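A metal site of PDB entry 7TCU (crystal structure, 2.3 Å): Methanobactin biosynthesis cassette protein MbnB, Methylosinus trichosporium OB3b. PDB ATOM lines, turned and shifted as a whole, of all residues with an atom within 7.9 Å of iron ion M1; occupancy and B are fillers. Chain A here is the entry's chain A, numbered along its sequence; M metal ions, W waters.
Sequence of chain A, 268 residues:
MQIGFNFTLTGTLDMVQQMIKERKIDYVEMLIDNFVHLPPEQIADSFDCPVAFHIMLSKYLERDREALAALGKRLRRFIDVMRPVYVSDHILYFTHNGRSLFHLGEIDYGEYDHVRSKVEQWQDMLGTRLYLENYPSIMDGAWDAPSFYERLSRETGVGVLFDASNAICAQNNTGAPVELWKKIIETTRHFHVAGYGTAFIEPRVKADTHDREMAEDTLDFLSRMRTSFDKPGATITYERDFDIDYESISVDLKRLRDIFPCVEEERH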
ATOM      1  N   ASN A   6       4.928   7.641  20.902  1.00  0.00           N
ATOM      2  CA  ASN A   6       5.943   8.588  20.460  1.00  0.00           C
ATOM      3  C   ASN A   6       5.350   9.990  20.396  1.00  0.00           C
ATOM      4  O   ASN A   6       4.305  10.213  19.773  1.00  0.00           O
ATOM      5  CB  ASN A   6       6.554   8.171  19.113  1.00  0.00           C
ATOM      6  CG  ASN A   6       5.639   8.422  17.898  1.00  0.00           C
ATOM      7  OD1 ASN A   6       4.452   8.083  17.903  1.00  0.00           O
ATOM      8  ND2 ASN A   6       6.214   9.002  16.844  1.00  0.00           N
ATOM      9  N   GLU A  29       7.966   8.281  24.511  1.00  0.00           N
ATOM     10  CA  GLU A  29       9.213   8.418  23.778  1.00  0.00           C
ATOM     11  C   GLU A  29       9.134   9.689  22.962  1.00  0.00           C
ATOM     12  O   GLU A  29       8.313   9.790  22.038  1.00  0.00           O
ATOM     13  CB  GLU A  29       9.461   7.215  22.871  1.00  0.00           C
ATOM     14  CG  GLU A  29      10.785   7.225  22.125  1.00  0.00           C
ATOM     15  CD  GLU A  29      10.895   6.014  21.178  1.00  0.00           C
ATOM     16  OE1 GLU A  29      10.851   4.849  21.679  1.00  0.00           O
ATOM     17  OE2 GLU A  29      10.958   6.225  19.946  1.00  0.00           O
ATOM     18  N   LEU A  31      10.633  12.544  20.322  1.00  0.00           N
ATOM     19  CA  LEU A  31      11.554  12.908  19.249  1.00  0.00           C
ATOM     20  C   LEU A  31      12.281  14.155  19.723  1.00  0.00           C
ATOM     21  O   LEU A  31      11.957  15.299  19.367  1.00  0.00           O
ATOM     22  CB  LEU A  31      10.798  13.110  17.951  1.00  0.00           C
ATOM     23  CG  LEU A  31      11.611  12.862  16.686  1.00  0.00           C
ATOM     24  CD1 LEU A  31      11.657  11.357  16.379  1.00  0.00           C
ATOM     25  CD2 LEU A  31      10.961  13.615  15.561  1.00  0.00           C
ATOM     26  N   HIS A  54      14.299   9.657  21.354  1.00  0.00           N
ATOM     27  CA  HIS A  54      14.553   9.304  19.972  1.00  0.00           C
ATOM     28  C   HIS A  54      15.081  10.540  19.241  1.00  0.00           C
ATOM     29  O   HIS A  54      14.452  11.596  19.283  1.00  0.00           O
ATOM     30  CB  HIS A  54      13.263   8.804  19.297  1.00  0.00           C
ATOM     31  CG  HIS A  54      13.479   7.875  18.148  1.00  0.00           C
ATOM     32  ND1 HIS A  54      14.451   6.905  18.149  1.00  0.00           N
ATOM     33  CD2 HIS A  54      12.813   7.740  16.980  1.00  0.00           C
ATOM     34  CE1 HIS A  54      14.402   6.230  17.016  1.00  0.00           C
ATOM     35  NE2 HIS A  54      13.406   6.713  16.289  1.00  0.00           N
ATOM     36  N   ILE A  55      16.238  10.424  18.593  1.00  0.00           N
ATOM     37  CA  ILE A  55      16.868  11.553  17.907  1.00  0.00           C
ATOM     38  C   ILE A  55      16.734  11.333  16.401  1.00  0.00           C
ATOM     39  O   ILE A  55      17.186  10.318  15.873  1.00  0.00           O
ATOM     40  CB  ILE A  55      18.344  11.700  18.322  1.00  0.00           C
ATOM     41  CG1 ILE A  55      18.435  11.986  19.820  1.00  0.00           C
ATOM     42  CG2 ILE A  55      19.038  12.764  17.508  1.00  0.00           C
ATOM     43  CD1 ILE A  55      19.645  11.331  20.480  1.00  0.00           C
ATOM     44  N   MET A  56      16.136  12.295  15.704  1.00  0.00           N
ATOM     45  CA  MET A  56      15.878  12.053  14.294  1.00  0.00           C
ATOM     46  C   MET A  56      16.848  12.760  13.365  1.00  0.00           C
ATOM     47  O   MET A  56      17.212  12.196  12.328  1.00  0.00           O
ATOM     48  CB  MET A  56      14.435  12.465  13.944  1.00  0.00           C
ATOM     49  CG  MET A  56      14.051  12.299  12.462  1.00  0.00           C
ATOM     50  SD  MET A  56      13.858  10.556  11.928  1.00  0.00           S
ATOM     51  CE  MET A  56      14.341  10.732  10.222  1.00  0.00           C
ATOM     52  N   SER A  88      18.206   7.062  21.646  1.00  0.00           N
ATOM     53  CA  SER A  88      18.224   6.336  20.384  1.00  0.00           C
ATOM     54  C   SER A  88      18.298   7.285  19.199  1.00  0.00           C
ATOM     55  O   SER A  88      17.922   8.466  19.280  1.00  0.00           O
ATOM     56  CB  SER A  88      17.001   5.431  20.227  1.00  0.00           C
ATOM     57  OG  SER A  88      15.787   6.151  20.345  1.00  0.00           O
ATOM     58  N   ASP A  89      18.802   6.734  18.104  1.00  0.00           N
ATOM     59  CA  ASP A  89      19.056   7.448  16.866  1.00  0.00           C
ATOM     60  C   ASP A  89      18.963   6.441  15.712  1.00  0.00           C
ATOM     61  O   ASP A  89      18.498   5.305  15.897  1.00  0.00           O
ATOM     62  CB  ASP A  89      20.419   8.141  16.965  1.00  0.00           C
ATOM     63  CG  ASP A  89      20.527   9.387  16.112  1.00  0.00           C
ATOM     64  OD1 ASP A  89      20.197   9.356  14.908  1.00  0.00           O
ATOM     65  OD2 ASP A  89      21.022  10.396  16.625  1.00  0.00           O
ATOM     66  N   HIS A  90      19.415   6.850  14.533  1.00  0.00           N
ATOM     67  CA  HIS A  90      19.177   6.128  13.304  1.00  0.00           C
ATOM     68  C   HIS A  90      20.459   5.902  12.526  1.00  0.00           C
ATOM     69  O   HIS A  90      21.513   6.447  12.857  1.00  0.00           O
ATOM     70  CB  HIS A  90      18.197   6.883  12.412  1.00  0.00           C
ATOM     71  CG  HIS A  90      16.856   7.099  13.021  1.00  0.00           C
ATOM     72  ND1 HIS A  90      16.626   8.061  13.988  1.00  0.00           N
ATOM     73  CD2 HIS A  90      15.686   6.450  12.829  1.00  0.00           C
ATOM     74  CE1 HIS A  90      15.351   8.004  14.346  1.00  0.00           C
ATOM     75  NE2 HIS A  90      14.756   7.045  13.652  1.00  0.00           N
ATOM     76  N   LEU A  92      20.910   6.548   8.697  1.00  0.00           N
ATOM     77  CA  LEU A  92      20.155   7.075   7.573  1.00  0.00           C
ATOM     78  C   LEU A  92      21.074   7.861   6.656  1.00  0.00           C
ATOM     79  O   LEU A  92      22.013   8.517   7.096  1.00  0.00           O
ATOM     80  CB  LEU A  92      18.992   7.970   8.064  1.00  0.00           C
ATOM     81  CG  LEU A  92      17.840   7.252   8.751  1.00  0.00           C
ATOM     82  CD1 LEU A  92      16.914   8.296   9.320  1.00  0.00           C
ATOM     83  CD2 LEU A  92      17.100   6.392   7.767  1.00  0.00           C
ATOM     84  N   GLU A 133      18.444   2.315  15.365  1.00  0.00           N
ATOM     85  CA  GLU A 133      17.266   1.716  14.780  1.00  0.00           C
ATOM     86  C   GLU A 133      17.580   1.065  13.433  1.00  0.00           C
ATOM     87  O   GLU A 133      18.473   1.502  12.700  1.00  0.00           O
ATOM     88  CB  GLU A 133      16.214   2.810  14.596  1.00  0.00           C
ATOM     89  CG  GLU A 133      14.847   2.383  14.098  1.00  0.00           C
ATOM     90  CD  GLU A 133      13.916   3.592  13.983  1.00  0.00           C
ATOM     91  OE1 GLU A 133      13.769   4.338  14.968  1.00  0.00           O
ATOM     92  OE2 GLU A 133      13.346   3.830  12.892  1.00  0.00           O
ATOM     93  N   ASN A 134      16.839   0.003  13.109  1.00  0.00           N
ATOM     94  CA  ASN A 134      16.951  -0.596  11.776  1.00  0.00           C
ATOM     95  C   ASN A 134      16.065   0.131  10.776  1.00  0.00           C
ATOM     96  O   ASN A 134      14.980   0.644  11.103  1.00  0.00           O
ATOM     97  CB  ASN A 134      16.581  -2.083  11.789  1.00  0.00           C
ATOM     98  CG  ASN A 134      15.262  -2.340  12.505  1.00  0.00           C
ATOM     99  OD1 ASN A 134      15.088  -1.930  13.667  1.00  0.00           O
ATOM    100  ND2 ASN A 134      14.326  -2.998  11.815  1.00  0.00           N
ATOM    101  N   LEU A 161      17.710  -0.499  18.693  1.00  0.00           N
ATOM    102  CA  LEU A 161      16.309  -0.184  18.915  1.00  0.00           C
ATOM    103  C   LEU A 161      15.572  -0.900  17.793  1.00  0.00           C
ATOM    104  O   LEU A 161      15.449  -0.386  16.690  1.00  0.00           O
ATOM    105  CB  LEU A 161      16.081   1.311  18.893  1.00  0.00           C
ATOM    106  CG  LEU A 161      14.627   1.717  19.093  1.00  0.00           C
ATOM    107  CD1 LEU A 161      14.064   0.963  20.258  1.00  0.00           C
ATOM    108  CD2 LEU A 161      14.542   3.215  19.328  1.00  0.00           C
ATOM    109  N   ASP A 163      12.990  -2.046  15.434  1.00  0.00           N
ATOM    110  CA  ASP A 163      11.694  -1.619  14.910  1.00  0.00           C
ATOM    111  C   ASP A 163      11.055  -2.786  14.165  1.00  0.00           C
ATOM    112  O   ASP A 163      11.468  -3.126  13.056  1.00  0.00           O
ATOM    113  CB  ASP A 163      11.871  -0.401  14.015  1.00  0.00           C
ATOM    114  CG  ASP A 163      10.516   0.274  13.670  1.00  0.00           C
ATOM    115  OD1 ASP A 163       9.682  -0.374  12.984  1.00  0.00           O
ATOM    116  OD2 ASP A 163      10.280   1.448  14.059  1.00  0.00           O
ATOM    117  N   ASN A 166       9.428  -1.988  10.602  1.00  0.00           N
ATOM    118  CA  ASN A 166      10.469  -1.788   9.592  1.00  0.00           C
ATOM    119  C   ASN A 166      11.058  -3.123   9.139  1.00  0.00           C
ATOM    120  O   ASN A 166      11.323  -3.312   7.949  1.00  0.00           O
ATOM    121  CB  ASN A 166      11.579  -0.896  10.147  1.00  0.00           C
ATOM    122  CG  ASN A 166      11.093   0.508  10.428  1.00  0.00           C
ATOM    123  OD1 ASN A 166       9.927   0.814  10.237  1.00  0.00           O
ATOM    124  ND2 ASN A 166      11.986   1.358  10.907  1.00  0.00           N
ATOM    125  N   HIS A 192      10.287  -0.903  18.727  1.00  0.00           N
ATOM    126  CA  HIS A 192       9.359   0.063  18.114  1.00  0.00           C
ATOM    127  C   HIS A 192       8.397  -0.737  17.248  1.00  0.00           C
ATOM    128  O   HIS A 192       8.802  -1.778  16.749  1.00  0.00           O
ATOM    129  CB  HIS A 192      10.095   0.922  17.115  1.00  0.00           C
ATOM    130  CG  HIS A 192      10.621   2.205  17.613  1.00  0.00           C
ATOM    131  ND1 HIS A 192      11.010   3.191  16.742  1.00  0.00           N
ATOM    132  CD2 HIS A 192      10.836   2.657  18.852  1.00  0.00           C
ATOM    133  CE1 HIS A 192      11.448   4.222  17.436  1.00  0.00           C
ATOM    134  NE2 HIS A 192      11.368   3.895  18.723  1.00  0.00           N
ATOM    135  N   ASP A 208       7.119   2.926   5.333  1.00  0.00           N
ATOM    136  CA  ASP A 208       7.014   3.128   6.795  1.00  0.00           C
ATOM    137  C   ASP A 208       6.258   4.427   7.114  1.00  0.00           C
ATOM    138  O   ASP A 208       6.801   5.413   7.639  1.00  0.00           O
ATOM    139  CB  ASP A 208       8.406   3.106   7.427  1.00  0.00           C
ATOM    140  CG  ASP A 208       9.290   4.272   6.976  1.00  0.00           C
ATOM    141  OD1 ASP A 208       9.560   4.410   5.759  1.00  0.00           O
ATOM    142  OD2 ASP A 208       9.737   5.051   7.833  1.00  0.00           O
ATOM    143  N   HIS A 210       3.708   5.069   9.233  1.00  0.00           N
ATOM    144  CA  HIS A 210       3.277   5.305  10.621  1.00  0.00           C
ATOM    145  C   HIS A 210       1.909   5.970  10.691  1.00  0.00           C
ATOM    146  O   HIS A 210       1.654   6.812  11.570  1.00  0.00           O
ATOM    147  CB  HIS A 210       4.304   6.133  11.385  1.00  0.00           C
ATOM    148  CG  HIS A 210       5.651   5.489  11.470  1.00  0.00           C
ATOM    149  ND1 HIS A 210       6.650   5.963  12.284  1.00  0.00           N
ATOM    150  CD2 HIS A 210       6.160   4.414  10.831  1.00  0.00           C
ATOM    151  CE1 HIS A 210       7.721   5.201  12.150  1.00  0.00           C
ATOM    152  NE2 HIS A 210       7.454   4.257  11.263  1.00  0.00           N
ATOM    153  N   GLU A 239       4.169   3.830  17.419  1.00  0.00           N
ATOM    154  CA  GLU A 239       4.435   5.104  16.742  1.00  0.00           C
ATOM    155  C   GLU A 239       3.321   5.463  15.770  1.00  0.00           C
ATOM    156  O   GLU A 239       3.010   4.651  14.912  1.00  0.00           O
ATOM    157  CB  GLU A 239       5.731   5.054  15.957  1.00  0.00           C
ATOM    158  CG  GLU A 239       6.938   4.679  16.787  1.00  0.00           C
ATOM    159  CD  GLU A 239       8.227   4.973  16.036  1.00  0.00           C
ATOM    160  OE1 GLU A 239       8.575   4.188  15.149  1.00  0.00           O
ATOM    161  OE2 GLU A 239       8.854   6.006  16.338  1.00  0.00           O
ATOM    162  N   ASP A 241       2.499   8.889  13.412  1.00  0.00           N
ATOM    163  CA  ASP A 241       2.861  10.239  13.025  1.00  0.00           C
ATOM    164  C   ASP A 241       1.796  10.909  12.191  1.00  0.00           C
ATOM    165  O   ASP A 241       1.814  12.132  12.038  1.00  0.00           O
ATOM    166  CB  ASP A 241       4.168  10.220  12.225  1.00  0.00           C
ATOM    167  CG  ASP A 241       5.257   9.431  12.924  1.00  0.00           C
ATOM    168  OD1 ASP A 241       5.453   9.603  14.145  1.00  0.00           O
ATOM    169  OD2 ASP A 241       5.930   8.626  12.249  1.00  0.00           O
HETATM  170 FE    FE M   1      12.915   6.394  14.131  1.00  0.00          FE
HETATM  171 FE    FE M   2      10.842   3.282  14.384  1.00  0.00          FE
HETATM  172 FE    FE M   3       8.581   2.238  11.261  1.00  0.00          FE
HETATM  173  O   HOH W   1      12.509   5.915  12.109  1.00  0.00           O
HETATM  174  O   HOH W   2      12.297   8.659  13.850  1.00  0.00           O
HETATM  175  O   HOH W   3      10.855   5.854  14.312  1.00  0.00           O
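ND1 of His 90 sits at hydrogen-bond distance from O of Ile 55 (3.0 Å).
A ring nitrogen (ND1) of His 54 lies within hydrogen-bond range of the side-chain hydroxyl (OG) of Ser 88.
N of Glu 133 sits at hydrogen-bond distance from O of Asp 89 (3.0 Å).
OE2 of Glu 133 sits at hydrogen-bond distance from ND2 of Asn 166.
Three residues have an atom within 4 Å of iron ion M1: His 54, His 90 and Glu 133.
The nearest printed residue that does not touch iron ion M1 is His 192 (4.2 Å).
Iron ion M1 is bound by NE2 of His 90 (2.0 Å), water W1 (2.1 Å), water W3 (2.1 Å), NE2 of His 54 (2.2 Å), water W2 (2.4 Å) and OE1 of Glu 133 (2.4 Å).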
